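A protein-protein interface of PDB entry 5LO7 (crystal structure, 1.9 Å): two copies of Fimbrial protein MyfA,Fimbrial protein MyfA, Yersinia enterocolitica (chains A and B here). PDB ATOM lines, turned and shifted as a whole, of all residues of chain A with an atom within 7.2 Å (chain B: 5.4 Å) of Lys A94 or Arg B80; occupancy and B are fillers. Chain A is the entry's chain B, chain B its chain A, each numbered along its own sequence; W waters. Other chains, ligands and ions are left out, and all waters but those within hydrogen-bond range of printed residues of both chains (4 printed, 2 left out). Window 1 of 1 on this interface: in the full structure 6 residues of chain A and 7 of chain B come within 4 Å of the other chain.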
ATOM      1  N   ILE A  12     -10.652  13.427 -22.839  1.00  0.00           N
ATOM      2  CA  ILE A  12     -11.052  13.707 -21.469  1.00  0.00           C
ATOM      3  C   ILE A  12      -9.819  13.972 -20.603  1.00  0.00           C
ATOM      4  O   ILE A  12      -8.819  13.258 -20.689  1.00  0.00           O
ATOM      5  CB  ILE A  12     -11.846  12.543 -20.858  1.00  0.00           C
ATOM      6  CG1 ILE A  12     -13.072  12.214 -21.707  1.00  0.00           C
ATOM      7  CG2 ILE A  12     -12.256  12.865 -19.432  1.00  0.00           C
ATOM      8  CD1 ILE A  12     -13.957  11.180 -21.074  1.00  0.00           C
ATOM      9  N   VAL A  13      -9.902  15.012 -19.782  1.00  0.00           N
ATOM     10  CA  VAL A  13      -8.847  15.346 -18.840  1.00  0.00           C
ATOM     11  C   VAL A  13      -9.381  15.044 -17.451  1.00  0.00           C
ATOM     12  O   VAL A  13     -10.583  15.142 -17.206  1.00  0.00           O
ATOM     13  CB  VAL A  13      -8.457  16.845 -18.962  1.00  0.00           C
ATOM     14  CG1 VAL A  13      -7.524  17.278 -17.850  1.00  0.00           C
ATOM     15  CG2 VAL A  13      -7.858  17.143 -20.330  1.00  0.00           C
ATOM     16  N   SER A  14      -8.490  14.689 -16.535  1.00  0.00           N
ATOM     17  CA  SER A  14      -8.881  14.470 -15.160  1.00  0.00           C
ATOM     18  C   SER A  14      -9.370  15.766 -14.525  1.00  0.00           C
ATOM     19  O   SER A  14      -8.860  16.847 -14.800  1.00  0.00           O
ATOM     20  CB  SER A  14      -7.695  13.980 -14.370  1.00  0.00           C
ATOM     21  OG  SER A  14      -6.780  15.038 -14.189  1.00  0.00           O
ATOM     22  N   GLY A  15     -10.358  15.648 -13.657  1.00  0.00           N
ATOM     23  CA  GLY A  15     -10.901  16.795 -12.973  1.00  0.00           C
ATOM     24  C   GLY A  15     -12.370  16.544 -12.799  1.00  0.00           C
ATOM     25  O   GLY A  15     -12.860  15.460 -13.118  1.00  0.00           O
ATOM     26  N   MET A  50     -16.497   1.596 -16.053  1.00  0.00           N
ATOM     27  CA  MET A  50     -15.187   1.418 -16.687  1.00  0.00           C
ATOM     28  C   MET A  50     -14.131   1.495 -15.598  1.00  0.00           C
ATOM     29  O   MET A  50     -14.209   2.328 -14.699  1.00  0.00           O
ATOM     30  CB  MET A  50     -14.914   2.479 -17.741  1.00  0.00           C
ATOM     31  CG  MET A  50     -14.972   3.909 -17.253  1.00  0.00           C
ATOM     32  SD  MET A  50     -14.461   5.034 -18.562  1.00  0.00           S
ATOM     33  CE  MET A  50     -14.087   6.554 -17.689  1.00  0.00           C
ATOM     34  N   VAL A  51     -13.140   0.626 -15.693  1.00  0.00           N
ATOM     35  CA  VAL A  51     -12.235   0.401 -14.595  1.00  0.00           C
ATOM     36  C   VAL A  51     -10.811   0.565 -15.089  1.00  0.00           C
ATOM     37  O   VAL A  51     -10.446  -0.004 -16.118  1.00  0.00           O
ATOM     38  CB  VAL A  51     -12.435  -1.011 -14.033  1.00  0.00           C
ATOM     39  CG1 VAL A  51     -11.583  -1.204 -12.814  1.00  0.00           C
ATOM     40  CG2 VAL A  51     -13.861  -1.232 -13.683  1.00  0.00           C
ATOM     41  N   SER A  52     -10.008   1.353 -14.368  1.00  0.00           N
ATOM     42  CA  SER A  52      -8.631   1.608 -14.783  1.00  0.00           C
ATOM     43  C   SER A  52      -7.724   0.497 -14.288  1.00  0.00           C
ATOM     44  O   SER A  52      -8.177  -0.408 -13.591  1.00  0.00           O
ATOM     45  CB  SER A  52      -8.131   2.971 -14.280  1.00  0.00           C
ATOM     46  OG  SER A  52      -7.960   2.986 -12.874  1.00  0.00           O
ATOM     47  N   ASP A  54      -5.423   0.645 -11.950  1.00  0.00           N
ATOM     48  CA  ASP A  54      -5.300   0.619 -10.499  1.00  0.00           C
ATOM     49  C   ASP A  54      -6.648   0.351  -9.846  1.00  0.00           C
ATOM     50  O   ASP A  54      -6.785   0.474  -8.632  1.00  0.00           O
ATOM     51  CB  ASP A  54      -4.663   1.896  -9.943  1.00  0.00           C
ATOM     52  CG  ASP A  54      -5.371   3.147 -10.371  1.00  0.00           C
ATOM     53  OD1 ASP A  54      -6.515   3.050 -10.833  1.00  0.00           O
ATOM     54  OD2 ASP A  54      -4.783   4.246 -10.212  1.00  0.00           O
ATOM     55  N   GLY A  55      -7.639  -0.014 -10.652  1.00  0.00           N
ATOM     56  CA  GLY A  55      -8.911  -0.444 -10.124  1.00  0.00           C
ATOM     57  C   GLY A  55      -9.936   0.658  -9.979  1.00  0.00           C
ATOM     58  O   GLY A  55     -11.054   0.378  -9.590  1.00  0.00           O
ATOM     59  N   THR A  56      -9.564   1.899 -10.278  1.00  0.00           N
ATOM     60  CA  THR A  56     -10.484   3.031 -10.115  1.00  0.00           C
ATOM     61  C   THR A  56     -11.692   2.864 -11.031  1.00  0.00           C
ATOM     62  O   THR A  56     -11.523   2.527 -12.202  1.00  0.00           O
ATOM     63  CB  THR A  56      -9.825   4.401 -10.432  1.00  0.00           C
ATOM     64  OG1 THR A  56      -8.669   4.593  -9.613  1.00  0.00           O
ATOM     65  CG2 THR A  56     -10.809   5.564 -10.168  1.00  0.00           C
ATOM     66  N   ARG A  57     -12.893   3.126 -10.513  1.00  0.00           N
ATOM     67  CA  ARG A  57     -14.120   2.934 -11.282  1.00  0.00           C
ATOM     68  C   ARG A  57     -14.814   4.262 -11.588  1.00  0.00           C
ATOM     69  O   ARG A  57     -14.850   5.161 -10.758  1.00  0.00           O
ATOM     70  CB  ARG A  57     -15.070   2.028 -10.511  1.00  0.00           C
ATOM     71  CG  ARG A  57     -14.380   0.850  -9.881  1.00  0.00           C
ATOM     72  CD  ARG A  57     -15.303   0.040  -9.006  1.00  0.00           C
ATOM     73  NE  ARG A  57     -16.375  -0.563  -9.786  1.00  0.00           N
ATOM     74  CZ  ARG A  57     -16.257  -1.673 -10.507  1.00  0.00           C
ATOM     75  NH1 ARG A  57     -15.107  -2.336 -10.554  1.00  0.00           N
ATOM     76  NH2 ARG A  57     -17.298  -2.123 -11.179  1.00  0.00           N
ATOM     77  N   VAL A  58     -15.357   4.378 -12.792  1.00  0.00           N
ATOM     78  CA  VAL A  58     -16.239   5.485 -13.138  1.00  0.00           C
ATOM     79  C   VAL A  58     -17.553   4.917 -13.719  1.00  0.00           C
ATOM     80  O   VAL A  58     -17.546   4.059 -14.600  1.00  0.00           O
ATOM     81  CB  VAL A  58     -15.567   6.440 -14.148  1.00  0.00           C
ATOM     82  CG1 VAL A  58     -16.476   7.615 -14.457  1.00  0.00           C
ATOM     83  CG2 VAL A  58     -14.226   6.927 -13.609  1.00  0.00           C
ATOM     84  N   ASP A  91     -18.915  14.411 -12.056  1.00  0.00           N
ATOM     85  CA  ASP A  91     -18.041  13.336 -11.606  1.00  0.00           C
ATOM     86  C   ASP A  91     -16.576  13.736 -11.703  1.00  0.00           C
ATOM     87  O   ASP A  91     -16.132  14.211 -12.735  1.00  0.00           O
ATOM     88  CB  ASP A  91     -18.271  12.070 -12.433  1.00  0.00           C
ATOM     89  CG  ASP A  91     -19.481  11.279 -11.978  1.00  0.00           C
ATOM     90  OD1 ASP A  91     -20.206  11.739 -11.059  1.00  0.00           O
ATOM     91  OD2 ASP A  91     -19.708  10.191 -12.558  1.00  0.00           O
ATOM     92  N   GLU A  92     -15.833  13.547 -10.618  1.00  0.00           N
ATOM     93  CA  GLU A  92     -14.409  13.822 -10.622  1.00  0.00           C
ATOM     94  C   GLU A  92     -13.706  12.612 -11.136  1.00  0.00           C
ATOM     95  O   GLU A  92     -13.825  11.541 -10.551  1.00  0.00           O
ATOM     96  CB  GLU A  92     -13.919  14.138  -9.233  1.00  0.00           C
ATOM     97  CG  GLU A  92     -14.388  15.480  -8.844  1.00  0.00           C
ATOM     98  CD  GLU A  92     -13.787  15.985  -7.561  1.00  0.00           C
ATOM     99  OE1 GLU A  92     -13.015  15.239  -6.914  1.00  0.00           O
ATOM    100  OE2 GLU A  92     -14.108  17.143  -7.217  1.00  0.00           O
ATOM    101  N   VAL A  93     -12.995  12.781 -12.246  1.00  0.00           N
ATOM    102  CA  VAL A  93     -12.362  11.659 -12.912  1.00  0.00           C
ATOM    103  C   VAL A  93     -10.849  11.742 -12.808  1.00  0.00           C
ATOM    104  O   VAL A  93     -10.243  12.801 -12.935  1.00  0.00           O
ATOM    105  CB  VAL A  93     -12.807  11.534 -14.373  1.00  0.00           C
ATOM    106  CG1 VAL A  93     -12.263  10.264 -14.972  1.00  0.00           C
ATOM    107  CG2 VAL A  93     -14.344  11.523 -14.461  1.00  0.00           C
ATOM    108  N   LYS A  94     -10.260  10.588 -12.547  1.00  0.00           N
ATOM    109  CA  LYS A  94      -8.849  10.480 -12.294  1.00  0.00           C
ATOM    110  C   LYS A  94      -8.204   9.449 -13.189  1.00  0.00           C
ATOM    111  O   LYS A  94      -8.431   9.462 -14.419  1.00  0.00           O
ATOM    112  CB  LYS A  94      -8.609  10.019 -10.873  1.00  0.00           C
ATOM    113  CG  LYS A  94      -9.029  10.932  -9.827  1.00  0.00           C
ATOM    114  CD  LYS A  94      -8.007  10.703  -8.738  1.00  0.00           C
ATOM    115  CE  LYS A  94      -8.283  11.517  -7.551  1.00  0.00           C
ATOM    116  NZ  LYS A  94      -8.221  10.638  -6.367  1.00  0.00           N
ATOM    117  N   ALA A  95      -7.424   8.546 -12.543  1.00  0.00           N
ATOM    118  CA  ALA A  95      -6.160   8.012 -13.091  1.00  0.00           C
ATOM    119  C   ALA A  95      -6.250   6.707 -13.833  1.00  0.00           C
ATOM    120  O   ALA A  95      -6.223   5.606 -13.232  1.00  0.00           O
ATOM    121  CB  ALA A  95      -4.980   8.040 -12.049  1.00  0.00           C
ATOM    122  N   GLY A  96      -6.435   6.876 -15.151  1.00  0.00           N
ATOM    123  CA  GLY A  96      -5.884   5.958 -16.108  1.00  0.00           C
ATOM    124  C   GLY A  96      -6.480   5.781 -17.474  1.00  0.00           C
ATOM    125  O   GLY A  96      -7.059   6.657 -18.129  1.00  0.00           O
ATOM    126  N   GLU A  97      -6.253   4.559 -17.908  1.00  0.00           N
ATOM    127  CA  GLU A  97      -6.774   4.040 -19.125  1.00  0.00           C
ATOM    128  C   GLU A  97      -7.862   3.126 -18.602  1.00  0.00           C
ATOM    129  O   GLU A  97      -7.586   2.143 -17.928  1.00  0.00           O
ATOM    130  CB  GLU A  97      -5.684   3.254 -19.862  1.00  0.00           C
ATOM    131  CG  GLU A  97      -4.494   4.101 -20.324  1.00  0.00           C
ATOM    132  CD  GLU A  97      -4.839   5.064 -21.450  1.00  0.00           C
ATOM    133  OE1 GLU A  97      -6.014   5.132 -21.851  1.00  0.00           O
ATOM    134  OE2 GLU A  97      -3.930   5.762 -21.945  1.00  0.00           O
ATOM    135  N   TYR A  98      -9.107   3.494 -18.856  1.00  0.00           N
ATOM    136  CA  TYR A  98     -10.234   2.841 -18.224  1.00  0.00           C
ATOM    137  C   TYR A  98     -10.875   1.903 -19.207  1.00  0.00           C
ATOM    138  O   TYR A  98     -11.273   2.322 -20.282  1.00  0.00           O
ATOM    139  CB  TYR A  98     -11.268   3.876 -17.837  1.00  0.00           C
ATOM    140  CG  TYR A  98     -10.880   4.762 -16.688  1.00  0.00           C
ATOM    141  CD1 TYR A  98     -11.269   4.445 -15.405  1.00  0.00           C
ATOM    142  CD2 TYR A  98     -10.151   5.924 -16.889  1.00  0.00           C
ATOM    143  CE1 TYR A  98     -10.941   5.241 -14.345  1.00  0.00           C
ATOM    144  CE2 TYR A  98      -9.824   6.741 -15.830  1.00  0.00           C
ATOM    145  CZ  TYR A  98     -10.223   6.386 -14.548  1.00  0.00           C
ATOM    146  OH  TYR A  98      -9.930   7.153 -13.443  1.00  0.00           O
ATOM    147  N   THR A 128      -9.057   6.620 -22.638  1.00  0.00           N
ATOM    148  CA  THR A 128      -8.019   7.328 -21.889  1.00  0.00           C
ATOM    149  C   THR A 128      -8.576   8.558 -21.214  1.00  0.00           C
ATOM    150  O   THR A 128      -9.366   9.309 -21.794  1.00  0.00           O
ATOM    151  CB  THR A 128      -6.909   7.848 -22.786  1.00  0.00           C
ATOM    152  OG1 THR A 128      -6.445   6.802 -23.642  1.00  0.00           O
ATOM    153  CG2 THR A 128      -5.760   8.376 -21.945  1.00  0.00           C
ATOM    154  N   VAL A 129      -8.146   8.773 -19.984  1.00  0.00           N
ATOM    155  CA  VAL A 129      -8.322  10.070 -19.376  1.00  0.00           C
ATOM    156  C   VAL A 129      -6.933  10.647 -19.148  1.00  0.00           C
ATOM    157  O   VAL A 129      -6.021   9.916 -18.744  1.00  0.00           O
ATOM    158  CB  VAL A 129      -9.175   9.979 -18.083  1.00  0.00           C
ATOM    159  CG1 VAL A 129      -9.339  11.354 -17.428  1.00  0.00           C
ATOM    160  CG2 VAL A 129     -10.536   9.376 -18.419  1.00  0.00           C
ATOM    161  N   LYS A 130      -6.782  11.912 -19.563  1.00  0.00           N
ATOM    162  CA  LYS A 130      -5.935  12.963 -18.951  1.00  0.00           C
ATOM    163  C   LYS A 130      -4.468  13.097 -19.358  1.00  0.00           C
ATOM    164  O   LYS A 130      -4.138  13.099 -20.537  1.00  0.00           O
ATOM    165  CB  LYS A 130      -6.050  12.968 -17.429  1.00  0.00           C
ATOM    166  CG  LYS A 130      -5.471  11.782 -16.837  1.00  0.00           C
ATOM    167  CD  LYS A 130      -5.275  11.750 -15.353  1.00  0.00           C
ATOM    168  CE  LYS A 130      -4.815  10.398 -15.060  1.00  0.00           C
ATOM    169  NZ  LYS A 130      -6.169   9.765 -15.278  1.00  0.00           N
ATOM    170  N   GLU B   4      -8.023  -0.194   2.380  1.00  0.00           N
ATOM    171  CA  GLU B   4      -6.901  -1.130   2.466  1.00  0.00           C
ATOM    172  C   GLU B   4      -5.710  -0.363   3.002  1.00  0.00           C
ATOM    173  O   GLU B   4      -5.375   0.696   2.494  1.00  0.00           O
ATOM    174  CB  GLU B   4      -6.529  -1.672   1.090  1.00  0.00           C
ATOM    175  CG  GLU B   4      -7.696  -2.239   0.293  1.00  0.00           C
ATOM    176  CD  GLU B   4      -7.494  -2.134  -1.224  1.00  0.00           C
ATOM    177  OE1 GLU B   4      -6.342  -2.225  -1.703  1.00  0.00           O
ATOM    178  OE2 GLU B   4      -8.499  -1.948  -1.939  1.00  0.00           O
ATOM    179  N   VAL B  27      -5.363   2.929   0.533  1.00  0.00           N
ATOM    180  CA  VAL B  27      -6.337   3.140  -0.524  1.00  0.00           C
ATOM    181  C   VAL B  27      -7.708   3.293   0.110  1.00  0.00           C
ATOM    182  O   VAL B  27      -8.103   2.464   0.909  1.00  0.00           O
ATOM    183  CB  VAL B  27      -6.391   1.941  -1.501  1.00  0.00           C
ATOM    184  CG1 VAL B  27      -7.432   2.183  -2.605  1.00  0.00           C
ATOM    185  CG2 VAL B  27      -5.027   1.680  -2.102  1.00  0.00           C
ATOM    186  N   MET B  28      -8.435   4.342  -0.252  1.00  0.00           N
ATOM    187  CA  MET B  28      -9.788   4.548   0.254  1.00  0.00           C
ATOM    188  C   MET B  28     -10.739   4.653  -0.931  1.00  0.00           C
ATOM    189  O   MET B  28     -10.455   5.383  -1.879  1.00  0.00           O
ATOM    190  CB  MET B  28      -9.849   5.815   1.100  1.00  0.00           C
ATOM    191  CG  MET B  28      -8.997   5.748   2.348  1.00  0.00           C
ATOM    192  SD  MET B  28      -8.852   7.324   3.228  1.00  0.00           S
ATOM    193  CE  MET B  28      -7.872   8.265   2.071  1.00  0.00           C
ATOM    194  N   SER B  29     -11.847   3.914  -0.883  1.00  0.00           N
ATOM    195  CA  SER B  29     -12.718   3.818  -2.045  1.00  0.00           C
ATOM    196  C   SER B  29     -14.203   3.747  -1.713  1.00  0.00           C
ATOM    197  O   SER B  29     -14.606   3.180  -0.697  1.00  0.00           O
ATOM    198  CB  SER B  29     -12.349   2.605  -2.889  1.00  0.00           C
ATOM    199  OG  SER B  29     -12.770   2.850  -4.208  1.00  0.00           O
ATOM    200  N   ASP B  30     -14.991   4.368  -2.578  1.00  0.00           N
ATOM    201  CA  ASP B  30     -16.420   4.274  -2.509  1.00  0.00           C
ATOM    202  C   ASP B  30     -17.014   4.800  -3.789  1.00  0.00           C
ATOM    203  O   ASP B  30     -16.645   5.870  -4.246  1.00  0.00           O
ATOM    204  CB  ASP B  30     -16.933   5.078  -1.326  1.00  0.00           C
ATOM    205  CG  ASP B  30     -18.387   4.838  -1.061  1.00  0.00           C
ATOM    206  OD1 ASP B  30     -18.886   3.776  -1.471  1.00  0.00           O
ATOM    207  OD2 ASP B  30     -19.027   5.703  -0.440  1.00  0.00           O
ATOM    208  N   ASP B  76     -11.834  14.734  -2.163  1.00  0.00           N
ATOM    209  CA  ASP B  76     -11.703  14.024  -3.416  1.00  0.00           C
ATOM    210  C   ASP B  76     -12.990  13.296  -3.695  1.00  0.00           C
ATOM    211  O   ASP B  76     -13.348  12.387  -2.961  1.00  0.00           O
ATOM    212  CB  ASP B  76     -10.562  13.029  -3.309  1.00  0.00           C
ATOM    213  CG  ASP B  76     -10.306  12.297  -4.593  1.00  0.00           C
ATOM    214  OD1 ASP B  76     -11.234  11.710  -5.186  1.00  0.00           O
ATOM    215  OD2 ASP B  76      -9.147  12.322  -5.012  1.00  0.00           O
ATOM    216  N   SER B  78     -13.711  11.464  -6.374  1.00  0.00           N
ATOM    217  CA  SER B  78     -13.594  10.308  -7.236  1.00  0.00           C
ATOM    218  C   SER B  78     -13.859   9.020  -6.428  1.00  0.00           C
ATOM    219  O   SER B  78     -13.997   9.052  -5.210  1.00  0.00           O
ATOM    220  CB  SER B  78     -12.213  10.285  -7.875  1.00  0.00           C
ATOM    221  OG  SER B  78     -11.262   9.782  -6.972  1.00  0.00           O
ATOM    222  N   GLU B  79     -13.920   7.891  -7.111  1.00  0.00           N
ATOM    223  CA  GLU B  79     -14.269   6.630  -6.470  1.00  0.00           C
ATOM    224  C   GLU B  79     -13.152   6.089  -5.584  1.00  0.00           C
ATOM    225  O   GLU B  79     -13.387   5.234  -4.743  1.00  0.00           O
ATOM    226  CB  GLU B  79     -14.611   5.588  -7.545  1.00  0.00           C
ATOM    227  CG  GLU B  79     -15.045   4.222  -7.017  1.00  0.00           C
ATOM    228  CD  GLU B  79     -13.925   3.207  -6.983  1.00  0.00           C
ATOM    229  OE1 GLU B  79     -12.898   3.402  -7.643  1.00  0.00           O
ATOM    230  OE2 GLU B  79     -14.070   2.197  -6.289  1.00  0.00           O
ATOM    231  N   ARG B  80     -11.937   6.590  -5.773  1.00  0.00           N
ATOM    232  CA  ARG B  80     -10.751   5.958  -5.193  1.00  0.00           C
ATOM    233  C   ARG B  80      -9.603   6.942  -5.033  1.00  0.00           C
ATOM    234  O   ARG B  80      -9.286   7.692  -5.955  1.00  0.00           O
ATOM    235  CB  ARG B  80     -10.279   4.809  -6.103  1.00  0.00           C
ATOM    236  CG  ARG B  80      -9.107   3.991  -5.572  1.00  0.00           C
ATOM    237  CD  ARG B  80      -8.930   2.644  -6.267  1.00  0.00           C
ATOM    238  NE  ARG B  80     -10.194   1.930  -6.511  1.00  0.00           N
ATOM    239  CZ  ARG B  80     -10.470   0.679  -6.118  1.00  0.00           C
ATOM    240  NH1 ARG B  80      -9.587  -0.061  -5.439  1.00  0.00           N
ATOM    241  NH2 ARG B  80     -11.651   0.155  -6.400  1.00  0.00           N
ATOM    242  N   VAL B  81      -8.996   6.926  -3.842  1.00  0.00           N
ATOM    243  CA  VAL B  81      -7.814   7.730  -3.524  1.00  0.00           C
ATOM    244  C   VAL B  81      -6.737   6.799  -2.974  1.00  0.00           C
ATOM    245  O   VAL B  81      -7.020   5.939  -2.149  1.00  0.00           O
ATOM    246  CB  VAL B  81      -8.130   8.837  -2.464  1.00  0.00           C
ATOM    247  CG1 VAL B  81      -6.838   9.509  -1.914  1.00  0.00           C
ATOM    248  CG2 VAL B  81      -9.092   9.870  -3.034  1.00  0.00           C
ATOM    249  N   GLU B  82      -5.506   6.984  -3.435  1.00  0.00           N
ATOM    250  CA  GLU B  82      -4.362   6.201  -2.997  1.00  0.00           C
ATOM    251  C   GLU B  82      -3.409   7.121  -2.233  1.00  0.00           C
ATOM    252  O   GLU B  82      -3.271   8.284  -2.607  1.00  0.00           O
ATOM    253  CB  GLU B  82      -3.655   5.630  -4.221  1.00  0.00           C
ATOM    254  CG  GLU B  82      -4.482   4.551  -4.968  1.00  0.00           C
ATOM    255  CD  GLU B  82      -5.285   5.047  -6.181  1.00  0.00           C
ATOM    256  OE1 GLU B  82      -5.246   6.254  -6.532  1.00  0.00           O
ATOM    257  OE2 GLU B  82      -5.977   4.189  -6.792  1.00  0.00           O
HETATM  258  O   HOH W   1      -7.732   6.762  -8.155  1.00  0.00           O
HETATM  259  O   HOH W   2      -5.592   9.212  -6.014  1.00  0.00           O
HETATM  260  O   HOH W   3     -14.070   7.956 -10.094  1.00  0.00           O
HETATM  261  O   HOH W   4     -10.624  14.175  -7.502  1.00  0.00           O
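No position is printed for both chains.
Of the 13 pairs that touch across the chains among the printed residues, none has its exchanged pair printed and touching as well.
The side-chain amino group of Lys A94 sits at hydrogen-bond distance from the backbone carbonyl oxygen of Arg B80, at 3.2 Å.
The side-chain carboxylate (OD1) of Asp B76 is in salt-bridge range of the side-chain amino group (NZ) of Lys A94, 3.4 Å away.
OG of Ser B78 lies within hydrogen-bond range of NZ of Lys A94 (3.2 Å).
The backbone carbonyl oxygen (O) of Gly A55 sits at hydrogen-bond distance from the guanidinium group (NH2) of Arg B80 (3.3 Å).
The side-chain carboxylate of Glu B79 sits at hydrogen-bond distance from the backbone NH of Arg A57 (2.9 Å).
The side-chain carboxylate (OD1) of Asp A54 is in hydrogen-bond range of the side-chain hydroxyl (OG) of Ser A52 (2.5 Å).
The side-chain amino group of Lys A130 is in hydrogen-bond range of the backbone carbonyl oxygen of Lys A94, 2.4 Å away.
The guanidinium group (NH2) of Arg B80 lies within salt-bridge range of the side-chain carboxylate (OE2) of Glu B79, 3.2 Å away.
O of Lys A94 lies close to OH of Tyr A98 (2.9 Å).
The backbone carbonyl oxygen of Glu B79 is in hydrogen-bond range of the backbone NH of Asp B30 (2.8 Å).
The backbone NH (N) of Thr A56 lies within hydrogen-bond range of the side-chain hydroxyl (OG) of Ser A52 (3.2 Å).
Water W4 bridges OE1 of Glu A92 and OD1 of Asp B76.
Water W1 lies within hydrogen-bond range of the side-chain hydroxyl (OG1) of Thr A56, the backbone carbonyl oxygen (O) of Arg B80 and the side-chain carboxylate (OE1) of Glu B82.
Water W3 bridges O of Arg A57 (3.0 Å) and N of Glu B79 (3.0 Å).
Water W2 lies within hydrogen-bond range of the side-chain amino group of Lys A94 and the side-chain carboxylate of Glu B82.
Along chain B the printed residues that touch a printed residue of chain A span positions 76 to 82.
Printed residues of chain A that touch a printed residue of chain B: Asp A54, Gly A55, Thr A56, Arg A57, Glu A92 and Lys A94.
Among the printed residues, 13 pairs touch across the chains.
Among the printed residues, Asp or Glu carboxylates within 4 Å of a Lys or Arg side-chain nitrogen of the other chain: Lys A94 with Asp B76 (2.4 Å).
Arg B80 touches Asp A54 (CD to O, 3.9 Å).
OE2 of Glu B82 touches OD2 of Asp A54, at 3.6 Å.
Thr A56 touches Glu B79 (CA to OE1, 3.5 Å).
CA of Thr A56 touches NE of Arg B80, 3.8 Å away.
Glu B82 touches Thr A56 (OE2 to OG1, 3.9 Å).
C of Asp B76 touches OE1 of Glu A92, 3.8 Å away.
O of Glu A92 touches CB of Ser B78 (3.4 Å).
Val B81 touches Lys A94 (CG2 to NZ, 3.5 Å).
Of chain B, only Asp B76 (2.4 Å), Ser B78 (3.2 Å), Arg B80 (3.2 Å) and Val B81 (3.5 Å) come within 4 Å of Lys A94.
Printed residues of chain A within 4 Å of Ser B78: Glu A92 (3.4 Å) and Lys A94 (3.2 Å).
Printed residues of chain A within 4 Å of Glu B82: Asp A54 (3.6 Å) and Thr A56 (3.9 Å).
Of the printed residues of chain B, Asp A54 touches Arg B80 and Glu B82.
Printed residues of chain B within 4 Å of Thr A56: Glu B79, Arg B80 and Glu B82.
Of the printed residues of chain A, Val B81 touches Lys A94 (3.5 Å).
Gly A15 touches none of the printed residues of chain B.
Thr A128 touches none of the printed residues of chain B.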
